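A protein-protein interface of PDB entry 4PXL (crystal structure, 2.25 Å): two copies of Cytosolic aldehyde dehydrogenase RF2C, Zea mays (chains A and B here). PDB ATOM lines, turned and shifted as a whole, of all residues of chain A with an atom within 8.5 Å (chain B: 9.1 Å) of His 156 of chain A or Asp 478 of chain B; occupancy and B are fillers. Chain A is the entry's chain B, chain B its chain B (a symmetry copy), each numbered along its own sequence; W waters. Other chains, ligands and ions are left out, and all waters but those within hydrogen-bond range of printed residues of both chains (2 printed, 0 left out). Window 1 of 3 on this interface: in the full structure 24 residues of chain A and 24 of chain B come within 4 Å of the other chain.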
ATOM      1  N   GLY A 150       2.883   0.514  19.294  1.00  0.00           N
ATOM      2  CA  GLY A 150       3.669   1.611  18.731  1.00  0.00           C
ATOM      3  C   GLY A 150       4.326   2.496  19.775  1.00  0.00           C
ATOM      4  O   GLY A 150       5.264   3.220  19.447  1.00  0.00           O
ATOM      5  N   ALA A 151       3.838   2.456  21.038  1.00  0.00           N
ATOM      6  CA  ALA A 151       4.385   3.249  22.140  1.00  0.00           C
ATOM      7  C   ALA A 151       5.523   2.519  22.839  1.00  0.00           C
ATOM      8  O   ALA A 151       6.342   3.160  23.502  1.00  0.00           O
ATOM      9  CB  ALA A 151       3.294   3.524  23.166  1.00  0.00           C
ATOM     10  N   ALA A 152       5.544   1.179  22.718  1.00  0.00           N
ATOM     11  CA  ALA A 152       6.447   0.295  23.425  1.00  0.00           C
ATOM     12  C   ALA A 152       7.928   0.588  23.269  1.00  0.00           C
ATOM     13  O   ALA A 152       8.658   0.451  24.245  1.00  0.00           O
ATOM     14  CB  ALA A 152       6.138  -1.160  23.093  1.00  0.00           C
ATOM     15  N   ASP A 153       8.354   1.045  22.086  1.00  0.00           N
ATOM     16  CA  ASP A 153       9.761   1.335  21.806  1.00  0.00           C
ATOM     17  C   ASP A 153      10.134   2.847  21.901  1.00  0.00           C
ATOM     18  O   ASP A 153      11.219   3.234  21.464  1.00  0.00           O
ATOM     19  CB  ASP A 153      10.129   0.754  20.428  1.00  0.00           C
ATOM     20  CG  ASP A 153       9.505   1.470  19.226  1.00  0.00           C
ATOM     21  OD1 ASP A 153       8.645   2.388  19.439  1.00  0.00           O
ATOM     22  OD2 ASP A 153       9.878   1.125  18.063  1.00  0.00           O
ATOM     23  N   LYS A 154       9.239   3.667  22.488  1.00  0.00           N
ATOM     24  CA  LYS A 154       9.301   5.132  22.598  1.00  0.00           C
ATOM     25  C   LYS A 154       9.127   5.644  24.023  1.00  0.00           C
ATOM     26  O   LYS A 154       8.886   6.840  24.194  1.00  0.00           O
ATOM     27  CB  LYS A 154       8.090   5.697  21.838  1.00  0.00           C
ATOM     28  CG  LYS A 154       8.366   5.909  20.409  1.00  0.00           C
ATOM     29  CD  LYS A 154       7.102   6.077  19.645  1.00  0.00           C
ATOM     30  CE  LYS A 154       7.432   5.719  18.214  1.00  0.00           C
ATOM     31  NZ  LYS A 154       7.299   4.262  17.944  1.00  0.00           N
ATOM     32  N   VAL A 155       9.136   4.753  25.025  1.00  0.00           N
ATOM     33  CA  VAL A 155       8.925   5.122  26.424  1.00  0.00           C
ATOM     34  C   VAL A 155      10.126   5.952  26.896  1.00  0.00           C
ATOM     35  O   VAL A 155      11.251   5.477  26.793  1.00  0.00           O
ATOM     36  CB  VAL A 155       8.716   3.848  27.290  1.00  0.00           C
ATOM     37  CG1 VAL A 155       8.699   4.180  28.779  1.00  0.00           C
ATOM     38  CG2 VAL A 155       7.450   3.099  26.880  1.00  0.00           C
ATOM     39  N   HIS A 156       9.891   7.171  27.402  1.00  0.00           N
ATOM     40  CA  HIS A 156      10.991   8.006  27.886  1.00  0.00           C
ATOM     41  C   HIS A 156      10.873   8.424  29.313  1.00  0.00           C
ATOM     42  O   HIS A 156       9.800   8.855  29.747  1.00  0.00           O
ATOM     43  CB  HIS A 156      11.128   9.317  27.074  1.00  0.00           C
ATOM     44  CG  HIS A 156      11.457   9.157  25.622  1.00  0.00           C
ATOM     45  ND1 HIS A 156      11.515  10.249  24.789  1.00  0.00           N
ATOM     46  CD2 HIS A 156      11.734   8.047  24.899  1.00  0.00           C
ATOM     47  CE1 HIS A 156      11.801   9.774  23.591  1.00  0.00           C
ATOM     48  NE2 HIS A 156      11.919   8.451  23.606  1.00  0.00           N
ATOM     49  N   GLY A 157      12.015   8.430  29.984  1.00  0.00           N
ATOM     50  CA  GLY A 157      12.203   9.026  31.298  1.00  0.00           C
ATOM     51  C   GLY A 157      12.839  10.379  31.047  1.00  0.00           C
ATOM     52  O   GLY A 157      12.883  10.857  29.906  1.00  0.00           O
ATOM     53  N   ALA A 158      13.364  11.000  32.082  1.00  0.00           N
ATOM     54  CA  ALA A 158      14.014  12.303  31.930  1.00  0.00           C
ATOM     55  C   ALA A 158      15.486  12.340  32.407  1.00  0.00           C
ATOM     56  O   ALA A 158      15.827  11.660  33.351  1.00  0.00           O
ATOM     57  CB  ALA A 158      13.220  13.338  32.709  1.00  0.00           C
ATOM     58  N   THR A 159      16.296  13.234  31.848  1.00  0.00           N
ATOM     59  CA  THR A 159      17.586  13.596  32.414  1.00  0.00           C
ATOM     60  C   THR A 159      17.264  14.928  33.094  1.00  0.00           C
ATOM     61  O   THR A 159      16.616  15.801  32.513  1.00  0.00           O
ATOM     62  CB  THR A 159      18.761  13.634  31.419  1.00  0.00           C
ATOM     63  OG1 THR A 159      18.482  14.561  30.388  1.00  0.00           O
ATOM     64  CG2 THR A 159      19.090  12.274  30.860  1.00  0.00           C
ATOM     65  N   THR A 170      15.753   9.882  35.428  1.00  0.00           N
ATOM     66  CA  THR A 170      14.718   8.957  35.820  1.00  0.00           C
ATOM     67  C   THR A 170      14.661   7.815  34.833  1.00  0.00           C
ATOM     68  O   THR A 170      14.869   8.025  33.638  1.00  0.00           O
ATOM     69  CB  THR A 170      13.353   9.630  36.040  1.00  0.00           C
ATOM     70  OG1 THR A 170      12.830  10.060  34.797  1.00  0.00           O
ATOM     71  CG2 THR A 170      13.398  10.779  37.055  1.00  0.00           C
ATOM     72  N   LEU A 171      14.389   6.605  35.341  1.00  0.00           N
ATOM     73  CA  LEU A 171      14.190   5.411  34.527  1.00  0.00           C
ATOM     74  C   LEU A 171      12.717   5.008  34.615  1.00  0.00           C
ATOM     75  O   LEU A 171      12.134   5.043  35.695  1.00  0.00           O
ATOM     76  CB  LEU A 171      15.075   4.239  35.001  1.00  0.00           C
ATOM     77  CG  LEU A 171      16.614   4.414  34.853  1.00  0.00           C
ATOM     78  CD1 LEU A 171      17.350   3.275  35.501  1.00  0.00           C
ATOM     79  CD2 LEU A 171      17.033   4.571  33.411  1.00  0.00           C
ATOM     80  N   LYS A 172      12.118   4.631  33.493  1.00  0.00           N
ATOM     81  CA  LYS A 172      10.751   4.139  33.466  1.00  0.00           C
ATOM     82  C   LYS A 172      10.792   2.613  33.408  1.00  0.00           C
ATOM     83  O   LYS A 172      11.195   2.035  32.400  1.00  0.00           O
ATOM     84  CB  LYS A 172       9.956   4.751  32.293  1.00  0.00           C
ATOM     85  CG  LYS A 172       9.786   6.246  32.418  1.00  0.00           C
ATOM     86  CD  LYS A 172       8.680   6.619  33.374  1.00  0.00           C
ATOM     87  CE  LYS A 172       8.544   8.116  33.432  1.00  0.00           C
ATOM     88  NZ  LYS A 172       7.304   8.548  34.133  1.00  0.00           N
ATOM     89  N   GLU A 173      10.464   1.966  34.522  1.00  0.00           N
ATOM     90  CA  GLU A 173      10.509   0.505  34.589  1.00  0.00           C
ATOM     91  C   GLU A 173       9.169  -0.145  34.761  1.00  0.00           C
ATOM     92  O   GLU A 173       8.275   0.472  35.350  1.00  0.00           O
ATOM     93  CB  GLU A 173      11.542  -0.046  35.595  1.00  0.00           C
ATOM     94  CG  GLU A 173      11.831   0.726  36.860  1.00  0.00           C
ATOM     95  CD  GLU A 173      12.809  -0.031  37.743  1.00  0.00           C
ATOM     96  OE1 GLU A 173      12.346  -0.894  38.525  1.00  0.00           O
ATOM     97  OE2 GLU A 173      14.036   0.185  37.602  1.00  0.00           O
ATOM     98  N   MET A 495      -1.339   8.038  26.360  1.00  0.00           N
ATOM     99  CA  MET A 495      -0.016   7.710  26.882  1.00  0.00           C
ATOM    100  C   MET A 495      -0.102   7.588  28.414  1.00  0.00           C
ATOM    101  O   MET A 495       0.728   6.908  29.018  1.00  0.00           O
ATOM    102  CB  MET A 495       0.997   8.811  26.490  1.00  0.00           C
ATOM    103  CG  MET A 495       1.295   8.880  25.010  1.00  0.00           C
ATOM    104  SD  MET A 495       1.896   7.323  24.249  1.00  0.00           S
ATOM    105  CE  MET A 495       3.497   7.107  25.099  1.00  0.00           C
ATOM    106  N   LEU A 498      -0.351   4.035  29.726  1.00  0.00           N
ATOM    107  CA  LEU A 498       0.962   3.399  29.679  1.00  0.00           C
ATOM    108  C   LEU A 498       1.766   3.806  30.920  1.00  0.00           C
ATOM    109  O   LEU A 498       2.262   2.926  31.617  1.00  0.00           O
ATOM    110  CB  LEU A 498       1.699   3.761  28.378  1.00  0.00           C
ATOM    111  CG  LEU A 498       3.057   3.099  28.150  1.00  0.00           C
ATOM    112  CD1 LEU A 498       2.937   1.577  28.027  1.00  0.00           C
ATOM    113  CD2 LEU A 498       3.697   3.629  26.880  1.00  0.00           C
ATOM    114  N   ASP A 499       1.768   5.115  31.267  1.00  0.00           N
ATOM    115  CA  ASP A 499       2.451   5.622  32.449  1.00  0.00           C
ATOM    116  C   ASP A 499       2.025   4.991  33.765  1.00  0.00           C
ATOM    117  O   ASP A 499       2.835   4.914  34.678  1.00  0.00           O
ATOM    118  CB  ASP A 499       2.439   7.164  32.531  1.00  0.00           C
ATOM    119  CG  ASP A 499       3.412   7.720  33.586  1.00  0.00           C
ATOM    120  OD1 ASP A 499       4.537   7.151  33.737  1.00  0.00           O
ATOM    121  OD2 ASP A 499       3.029   8.672  34.308  1.00  0.00           O
ATOM    122  N   LEU A 502       4.187   1.851  34.644  1.00  0.00           N
ATOM    123  CA  LEU A 502       5.599   2.146  34.704  1.00  0.00           C
ATOM    124  C   LEU A 502       5.906   2.870  36.005  1.00  0.00           C
ATOM    125  O   LEU A 502       5.218   3.812  36.379  1.00  0.00           O
ATOM    126  CB  LEU A 502       6.118   2.982  33.481  1.00  0.00           C
ATOM    127  CG  LEU A 502       6.029   2.285  32.103  1.00  0.00           C
ATOM    128  CD1 LEU A 502       5.841   3.264  30.998  1.00  0.00           C
ATOM    129  CD2 LEU A 502       7.216   1.349  31.823  1.00  0.00           C
ATOM    130  N   GLN A 503       6.964   2.455  36.660  1.00  0.00           N
ATOM    131  CA  GLN A 503       7.451   3.120  37.833  1.00  0.00           C
ATOM    132  C   GLN A 503       8.536   4.073  37.392  1.00  0.00           C
ATOM    133  O   GLN A 503       9.236   3.804  36.415  1.00  0.00           O
ATOM    134  CB  GLN A 503       8.044   2.081  38.772  1.00  0.00           C
ATOM    135  CG  GLN A 503       7.367   2.161  40.125  1.00  0.00           C
ATOM    136  CD  GLN A 503       6.980   0.831  40.683  1.00  0.00           C
ATOM    137  OE1 GLN A 503       6.165   0.767  41.598  1.00  0.00           O
ATOM    138  NE2 GLN A 503       7.557  -0.260  40.170  1.00  0.00           N
ATOM    139  N   THR A 504       8.669   5.191  38.097  1.00  0.00           N
ATOM    140  CA  THR A 504       9.716   6.184  37.870  1.00  0.00           C
ATOM    141  C   THR A 504      10.791   5.921  38.928  1.00  0.00           C
ATOM    142  O   THR A 504      10.486   5.927  40.120  1.00  0.00           O
ATOM    143  CB  THR A 504       9.154   7.627  37.979  1.00  0.00           C
ATOM    144  OG1 THR A 504       8.223   7.832  36.943  1.00  0.00           O
ATOM    145  CG2 THR A 504      10.249   8.708  37.868  1.00  0.00           C
ATOM    146  N   HIS B 143      12.871  -1.425  10.357  1.00  0.00           N
ATOM    147  CA  HIS B 143      12.725  -1.182  11.798  1.00  0.00           C
ATOM    148  C   HIS B 143      12.524   0.328  12.070  1.00  0.00           C
ATOM    149  O   HIS B 143      11.598   0.702  12.807  1.00  0.00           O
ATOM    150  CB  HIS B 143      13.946  -1.756  12.559  1.00  0.00           C
ATOM    151  CG  HIS B 143      14.009  -1.447  14.030  1.00  0.00           C
ATOM    152  ND1 HIS B 143      15.022  -1.956  14.817  1.00  0.00           N
ATOM    153  CD2 HIS B 143      13.215  -0.662  14.811  1.00  0.00           C
ATOM    154  CE1 HIS B 143      14.804  -1.490  16.037  1.00  0.00           C
ATOM    155  NE2 HIS B 143      13.728  -0.709  16.080  1.00  0.00           N
ATOM    156  N   LEU B 144      13.350   1.182  11.448  1.00  0.00           N
ATOM    157  CA  LEU B 144      13.215   2.627  11.620  1.00  0.00           C
ATOM    158  C   LEU B 144      11.853   3.143  11.084  1.00  0.00           C
ATOM    159  O   LEU B 144      11.197   3.957  11.743  1.00  0.00           O
ATOM    160  CB  LEU B 144      14.379   3.347  10.957  1.00  0.00           C
ATOM    161  CG  LEU B 144      14.437   4.850  11.176  1.00  0.00           C
ATOM    162  CD1 LEU B 144      14.923   5.179  12.535  1.00  0.00           C
ATOM    163  CD2 LEU B 144      15.398   5.472  10.239  1.00  0.00           C
ATOM    164  N   TYR B 147       9.288   2.420  13.626  1.00  0.00           N
ATOM    165  CA  TYR B 147       9.369   3.381  14.718  1.00  0.00           C
ATOM    166  C   TYR B 147       8.499   4.621  14.405  1.00  0.00           C
ATOM    167  O   TYR B 147       7.700   5.012  15.243  1.00  0.00           O
ATOM    168  CB  TYR B 147      10.820   3.759  14.998  1.00  0.00           C
ATOM    169  CG  TYR B 147      10.974   4.798  16.089  1.00  0.00           C
ATOM    170  CD1 TYR B 147      11.003   6.153  15.787  1.00  0.00           C
ATOM    171  CD2 TYR B 147      11.070   4.426  17.423  1.00  0.00           C
ATOM    172  CE1 TYR B 147      11.214   7.114  16.776  1.00  0.00           C
ATOM    173  CE2 TYR B 147      11.252   5.377  18.423  1.00  0.00           C
ATOM    174  CZ  TYR B 147      11.316   6.725  18.092  1.00  0.00           C
ATOM    175  OH  TYR B 147      11.485   7.690  19.046  1.00  0.00           O
ATOM    176  N   TYR B 148       8.617   5.189  13.192  1.00  0.00           N
ATOM    177  CA  TYR B 148       7.821   6.361  12.774  1.00  0.00           C
ATOM    178  C   TYR B 148       6.393   6.051  12.504  1.00  0.00           C
ATOM    179  O   TYR B 148       5.542   6.876  12.820  1.00  0.00           O
ATOM    180  CB  TYR B 148       8.477   7.133  11.625  1.00  0.00           C
ATOM    181  CG  TYR B 148       9.760   7.761  12.111  1.00  0.00           C
ATOM    182  CD1 TYR B 148       9.737   8.810  13.038  1.00  0.00           C
ATOM    183  CD2 TYR B 148      10.997   7.222  11.764  1.00  0.00           C
ATOM    184  CE1 TYR B 148      10.911   9.315  13.579  1.00  0.00           C
ATOM    185  CE2 TYR B 148      12.176   7.727  12.299  1.00  0.00           C
ATOM    186  CZ  TYR B 148      12.123   8.771  13.206  1.00  0.00           C
ATOM    187  OH  TYR B 148      13.246   9.302  13.735  1.00  0.00           O
ATOM    188  N   ALA B 151       4.797   6.264  15.712  1.00  0.00           N
ATOM    189  CA  ALA B 151       4.769   7.628  16.246  1.00  0.00           C
ATOM    190  C   ALA B 151       3.653   8.449  15.616  1.00  0.00           C
ATOM    191  O   ALA B 151       3.230   9.449  16.199  1.00  0.00           O
ATOM    192  CB  ALA B 151       6.094   8.321  15.955  1.00  0.00           C
ATOM    193  N   ALA B 474      26.260   3.068  18.038  1.00  0.00           N
ATOM    194  CA  ALA B 474      25.088   2.698  18.829  1.00  0.00           C
ATOM    195  C   ALA B 474      23.869   3.509  18.399  1.00  0.00           C
ATOM    196  O   ALA B 474      23.220   4.158  19.222  1.00  0.00           O
ATOM    197  CB  ALA B 474      25.380   2.878  20.313  1.00  0.00           C
ATOM    198  N   PHE B 475      23.564   3.487  17.093  1.00  0.00           N
ATOM    199  CA  PHE B 475      22.401   4.179  16.539  1.00  0.00           C
ATOM    200  C   PHE B 475      21.181   3.404  16.972  1.00  0.00           C
ATOM    201  O   PHE B 475      21.259   2.193  17.159  1.00  0.00           O
ATOM    202  CB  PHE B 475      22.437   4.198  15.007  1.00  0.00           C
ATOM    203  CG  PHE B 475      23.558   4.998  14.414  1.00  0.00           C
ATOM    204  CD1 PHE B 475      23.471   6.378  14.319  1.00  0.00           C
ATOM    205  CD2 PHE B 475      24.681   4.369  13.891  1.00  0.00           C
ATOM    206  CE1 PHE B 475      24.505   7.119  13.736  1.00  0.00           C
ATOM    207  CE2 PHE B 475      25.713   5.110  13.321  1.00  0.00           C
ATOM    208  CZ  PHE B 475      25.614   6.482  13.242  1.00  0.00           C
ATOM    209  N   ASP B 476      20.065   4.089  17.124  1.00  0.00           N
ATOM    210  CA  ASP B 476      18.810   3.466  17.521  1.00  0.00           C
ATOM    211  C   ASP B 476      17.685   4.351  17.029  1.00  0.00           C
ATOM    212  O   ASP B 476      17.772   5.580  17.174  1.00  0.00           O
ATOM    213  CB  ASP B 476      18.723   3.339  19.058  1.00  0.00           C
ATOM    214  CG  ASP B 476      17.603   2.426  19.512  1.00  0.00           C
ATOM    215  OD1 ASP B 476      16.434   2.909  19.606  1.00  0.00           O
ATOM    216  OD2 ASP B 476      17.864   1.216  19.683  1.00  0.00           O
ATOM    217  N   PRO B 477      16.591   3.757  16.495  1.00  0.00           N
ATOM    218  CA  PRO B 477      15.455   4.580  16.072  1.00  0.00           C
ATOM    219  C   PRO B 477      14.996   5.613  17.107  1.00  0.00           C
ATOM    220  O   PRO B 477      14.558   6.689  16.718  1.00  0.00           O
ATOM    221  CB  PRO B 477      14.380   3.531  15.785  1.00  0.00           C
ATOM    222  CG  PRO B 477      15.169   2.352  15.297  1.00  0.00           C
ATOM    223  CD  PRO B 477      16.342   2.319  16.221  1.00  0.00           C
ATOM    224  N   ASP B 478      15.103   5.301  18.412  1.00  0.00           N
ATOM    225  CA  ASP B 478      14.674   6.192  19.507  1.00  0.00           C
ATOM    226  C   ASP B 478      15.693   7.262  19.922  1.00  0.00           C
ATOM    227  O   ASP B 478      15.350   8.188  20.661  1.00  0.00           O
ATOM    228  CB  ASP B 478      14.170   5.388  20.730  1.00  0.00           C
ATOM    229  CG  ASP B 478      13.357   6.218  21.728  1.00  0.00           C
ATOM    230  OD1 ASP B 478      12.473   7.006  21.279  1.00  0.00           O
ATOM    231  OD2 ASP B 478      13.618   6.101  22.953  1.00  0.00           O
ATOM    232  N   ALA B 479      16.929   7.146  19.422  1.00  0.00           N
ATOM    233  CA  ALA B 479      18.018   8.050  19.758  1.00  0.00           C
ATOM    234  C   ALA B 479      18.297   9.110  18.684  1.00  0.00           C
ATOM    235  O   ALA B 479      18.703   8.758  17.565  1.00  0.00           O
ATOM    236  CB  ALA B 479      19.285   7.249  20.089  1.00  0.00           C
ATOM    237  N   PRO B 480      18.123  10.420  19.015  1.00  0.00           N
ATOM    238  CA  PRO B 480      18.410  11.472  18.010  1.00  0.00           C
ATOM    239  C   PRO B 480      19.886  11.498  17.642  1.00  0.00           C
ATOM    240  O   PRO B 480      20.732  11.258  18.492  1.00  0.00           O
ATOM    241  CB  PRO B 480      17.985  12.781  18.691  1.00  0.00           C
ATOM    242  CG  PRO B 480      17.866  12.485  20.133  1.00  0.00           C
ATOM    243  CD  PRO B 480      17.634  10.998  20.290  1.00  0.00           C
ATOM    244  N   PHE B 481      20.179  11.767  16.364  1.00  0.00           N
ATOM    245  CA  PHE B 481      21.528  11.804  15.828  1.00  0.00           C
ATOM    246  C   PHE B 481      21.737  13.067  15.000  1.00  0.00           C
ATOM    247  O   PHE B 481      21.001  13.339  14.061  1.00  0.00           O
ATOM    248  CB  PHE B 481      21.796  10.541  15.007  1.00  0.00           C
ATOM    249  CG  PHE B 481      23.151  10.555  14.339  1.00  0.00           C
ATOM    250  CD1 PHE B 481      24.316  10.377  15.087  1.00  0.00           C
ATOM    251  CD2 PHE B 481      23.271  10.837  12.977  1.00  0.00           C
ATOM    252  CE1 PHE B 481      25.564  10.439  14.471  1.00  0.00           C
ATOM    253  CE2 PHE B 481      24.522  10.927  12.374  1.00  0.00           C
ATOM    254  CZ  PHE B 481      25.656  10.701  13.116  1.00  0.00           C
ATOM    255  N   ASP B 492      18.470  13.470  12.908  1.00  0.00           N
ATOM    256  CA  ASP B 492      17.923  12.318  12.197  1.00  0.00           C
ATOM    257  C   ASP B 492      17.753  11.284  13.305  1.00  0.00           C
ATOM    258  O   ASP B 492      18.521  11.293  14.273  1.00  0.00           O
ATOM    259  CB  ASP B 492      18.888  11.794  11.111  1.00  0.00           C
ATOM    260  CG  ASP B 492      18.885  12.591   9.820  1.00  0.00           C
ATOM    261  OD1 ASP B 492      17.798  13.085   9.420  1.00  0.00           O
ATOM    262  OD2 ASP B 492      19.965  12.724   9.206  1.00  0.00           O
ATOM    263  N   MET B 493      16.731  10.429  13.208  1.00  0.00           N
ATOM    264  CA  MET B 493      16.401   9.424  14.244  1.00  0.00           C
ATOM    265  C   MET B 493      15.796  10.066  15.497  1.00  0.00           C
ATOM    266  O   MET B 493      15.896  11.297  15.701  1.00  0.00           O
ATOM    267  CB  MET B 493      17.575   8.457  14.552  1.00  0.00           C
ATOM    268  CG  MET B 493      18.118   7.780  13.316  1.00  0.00           C
ATOM    269  SD  MET B 493      19.530   6.697  13.624  1.00  0.00           S
ATOM    270  CE  MET B 493      18.696   5.126  13.636  1.00  0.00           C
ATOM    271  N   GLY B 494      15.107   9.244  16.289  1.00  0.00           N
ATOM    272  CA  GLY B 494      14.423   9.716  17.487  1.00  0.00           C
ATOM    273  C   GLY B 494      13.155  10.476  17.142  1.00  0.00           C
ATOM    274  O   GLY B 494      12.811  10.646  15.966  1.00  0.00           O
ATOM    275  N   MET B 495      12.443  10.933  18.167  1.00  0.00           N
ATOM    276  CA  MET B 495      11.234  11.735  18.004  1.00  0.00           C
ATOM    277  C   MET B 495      11.621  13.105  17.419  1.00  0.00           C
ATOM    278  O   MET B 495      10.784  13.758  16.794  1.00  0.00           O
ATOM    279  CB  MET B 495      10.530  11.917  19.369  1.00  0.00           C
ATOM    280  CG  MET B 495       9.943  10.646  19.937  1.00  0.00           C
ATOM    281  SD  MET B 495       8.755   9.767  18.849  1.00  0.00           S
ATOM    282  CE  MET B 495       7.394  10.979  18.756  1.00  0.00           C
ATOM    283  N   ASP B 496      12.888  13.541  17.634  1.00  0.00           N
ATOM    284  CA  ASP B 496      13.424  14.832  17.150  1.00  0.00           C
ATOM    285  C   ASP B 496      13.325  14.958  15.638  1.00  0.00           C
ATOM    286  O   ASP B 496      13.029  16.051  15.149  1.00  0.00           O
ATOM    287  CB  ASP B 496      14.882  15.013  17.603  1.00  0.00           C
ATOM    288  CG  ASP B 496      15.096  14.858  19.107  1.00  0.00           C
ATOM    289  OD1 ASP B 496      14.707  13.795  19.660  1.00  0.00           O
ATOM    290  OD2 ASP B 496      15.688  15.772  19.723  1.00  0.00           O
ATOM    291  N   ALA B 497      13.567  13.840  14.901  1.00  0.00           N
ATOM    292  CA  ALA B 497      13.509  13.806  13.437  1.00  0.00           C
ATOM    293  C   ALA B 497      12.072  14.059  12.976  1.00  0.00           C
ATOM    294  O   ALA B 497      11.856  14.801  12.010  1.00  0.00           O
ATOM    295  CB  ALA B 497      14.019  12.475  12.905  1.00  0.00           C
HETATM  296  O   HOH W   1      12.614   0.821  18.046  1.00  0.00           O
HETATM  297  O   HOH W   2      13.588   1.712  20.262  1.00  0.00           O
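OD2 of Asp 153 of chain A touches CD2 of Tyr 147 of chain B (3.6 Å). Asp 478 of chain B touches Asp 153 of chain A (CG to O, 3.7 Å). CE of Lys 154 of chain A touches N of Ala 151 of chain B, 3.7 Å away. Lys 154 of chain A touches Asp 478 of chain B.
Printed residues of chain B within 4 Å of Asp 153 of chain A: Tyr 147 (3.6 Å) and Asp 478 (3.7 Å). Printed residues of chain B within 4 Å of Lys 154 of chain A: Tyr 147 (2.8 Å), Ala 151 (3.7 Å) and Asp 478 (3.9 Å). His 156 of chain A touches just one residue of chain B: Asp 478 (2.8 Å). Gly 157 of chain A touches none of the printed residues of chain B. Of the printed residues of chain A, Tyr 147 of chain B touches Asp 153 (3.6 Å) and Lys 154 (2.8 Å). Of the printed residues of chain A, Ala 151 of chain B touches Lys 154. No residue of chain A comes within 4 Å of Pro 477 of chain B. Of chain A, only Asp 153, Lys 154 and His 156 come within 4 Å of Asp 478 of chain B. No residue of chain A comes within 4 Å of Ala 479 of chain B. The nearest residue of chain B that does not touch His 156 of chain A is Met 495 of chain B (4.2 Å). The nearest residue of chain A that does not touch Asp 478 of chain B is Val 155 of chain A (4.6 Å).
2 positions are printed for both chains.
Printed residues of chain A that touch a printed residue of chain B: Asp 153, Lys 154 and His 156. Among the printed residues, 6 pairs touch across the chains. Among the printed residues, no Asp or Glu carboxylate lies within 4 Å of a Lys or Arg side-chain nitrogen of the other chain.
Water W1 bridges NE2 of His 143 of chain B (2.7 Å) and OD2 of Asp 153 of chain A (2.8 Å). Water W2 bridges O of Asp 153 of chain A (3.1 Å) and OD1 of Asp 476 of chain B (3.2 Å).
A ring nitrogen (NE2) of His 156 of chain A is in hydrogen-bond range of the side-chain carboxylate of Asp 478 of chain B, at 2.8 Å. The side-chain amino group (NZ) of Lys 154 of chain A sits at hydrogen-bond distance from the backbone carbonyl oxygen (O) of Tyr 147 of chain B, 2.8 Å away.
O of Lys 154 of chain A sits close to NE2 of His 156 of chain A, at 3.5 Å. N of Asp 478 of chain B lies within hydrogen-bond range of OD1 of Asp 476 of chain B (3.0 Å). The side-chain hydroxyl (OH) of Tyr 147 of chain B sits at hydrogen-bond distance from the side-chain carboxylate (OD1) of Asp 478 of chain B (2.5 Å). The backbone carbonyl oxygen (O) of Gly 150 of chain A is in hydrogen-bond range of the side-chain amino group (NZ) of Lys 154 of chain A (2.7 Å). The side-chain hydroxyl (OH) of Tyr 147 of chain B lies within hydrogen-bond range of the side-chain sulfur (SD) of Met 495 of chain B. OD1 of Asp 153 of chain A lies within salt-bridge range of NZ of Lys 154 of chain A (2.7 Å).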
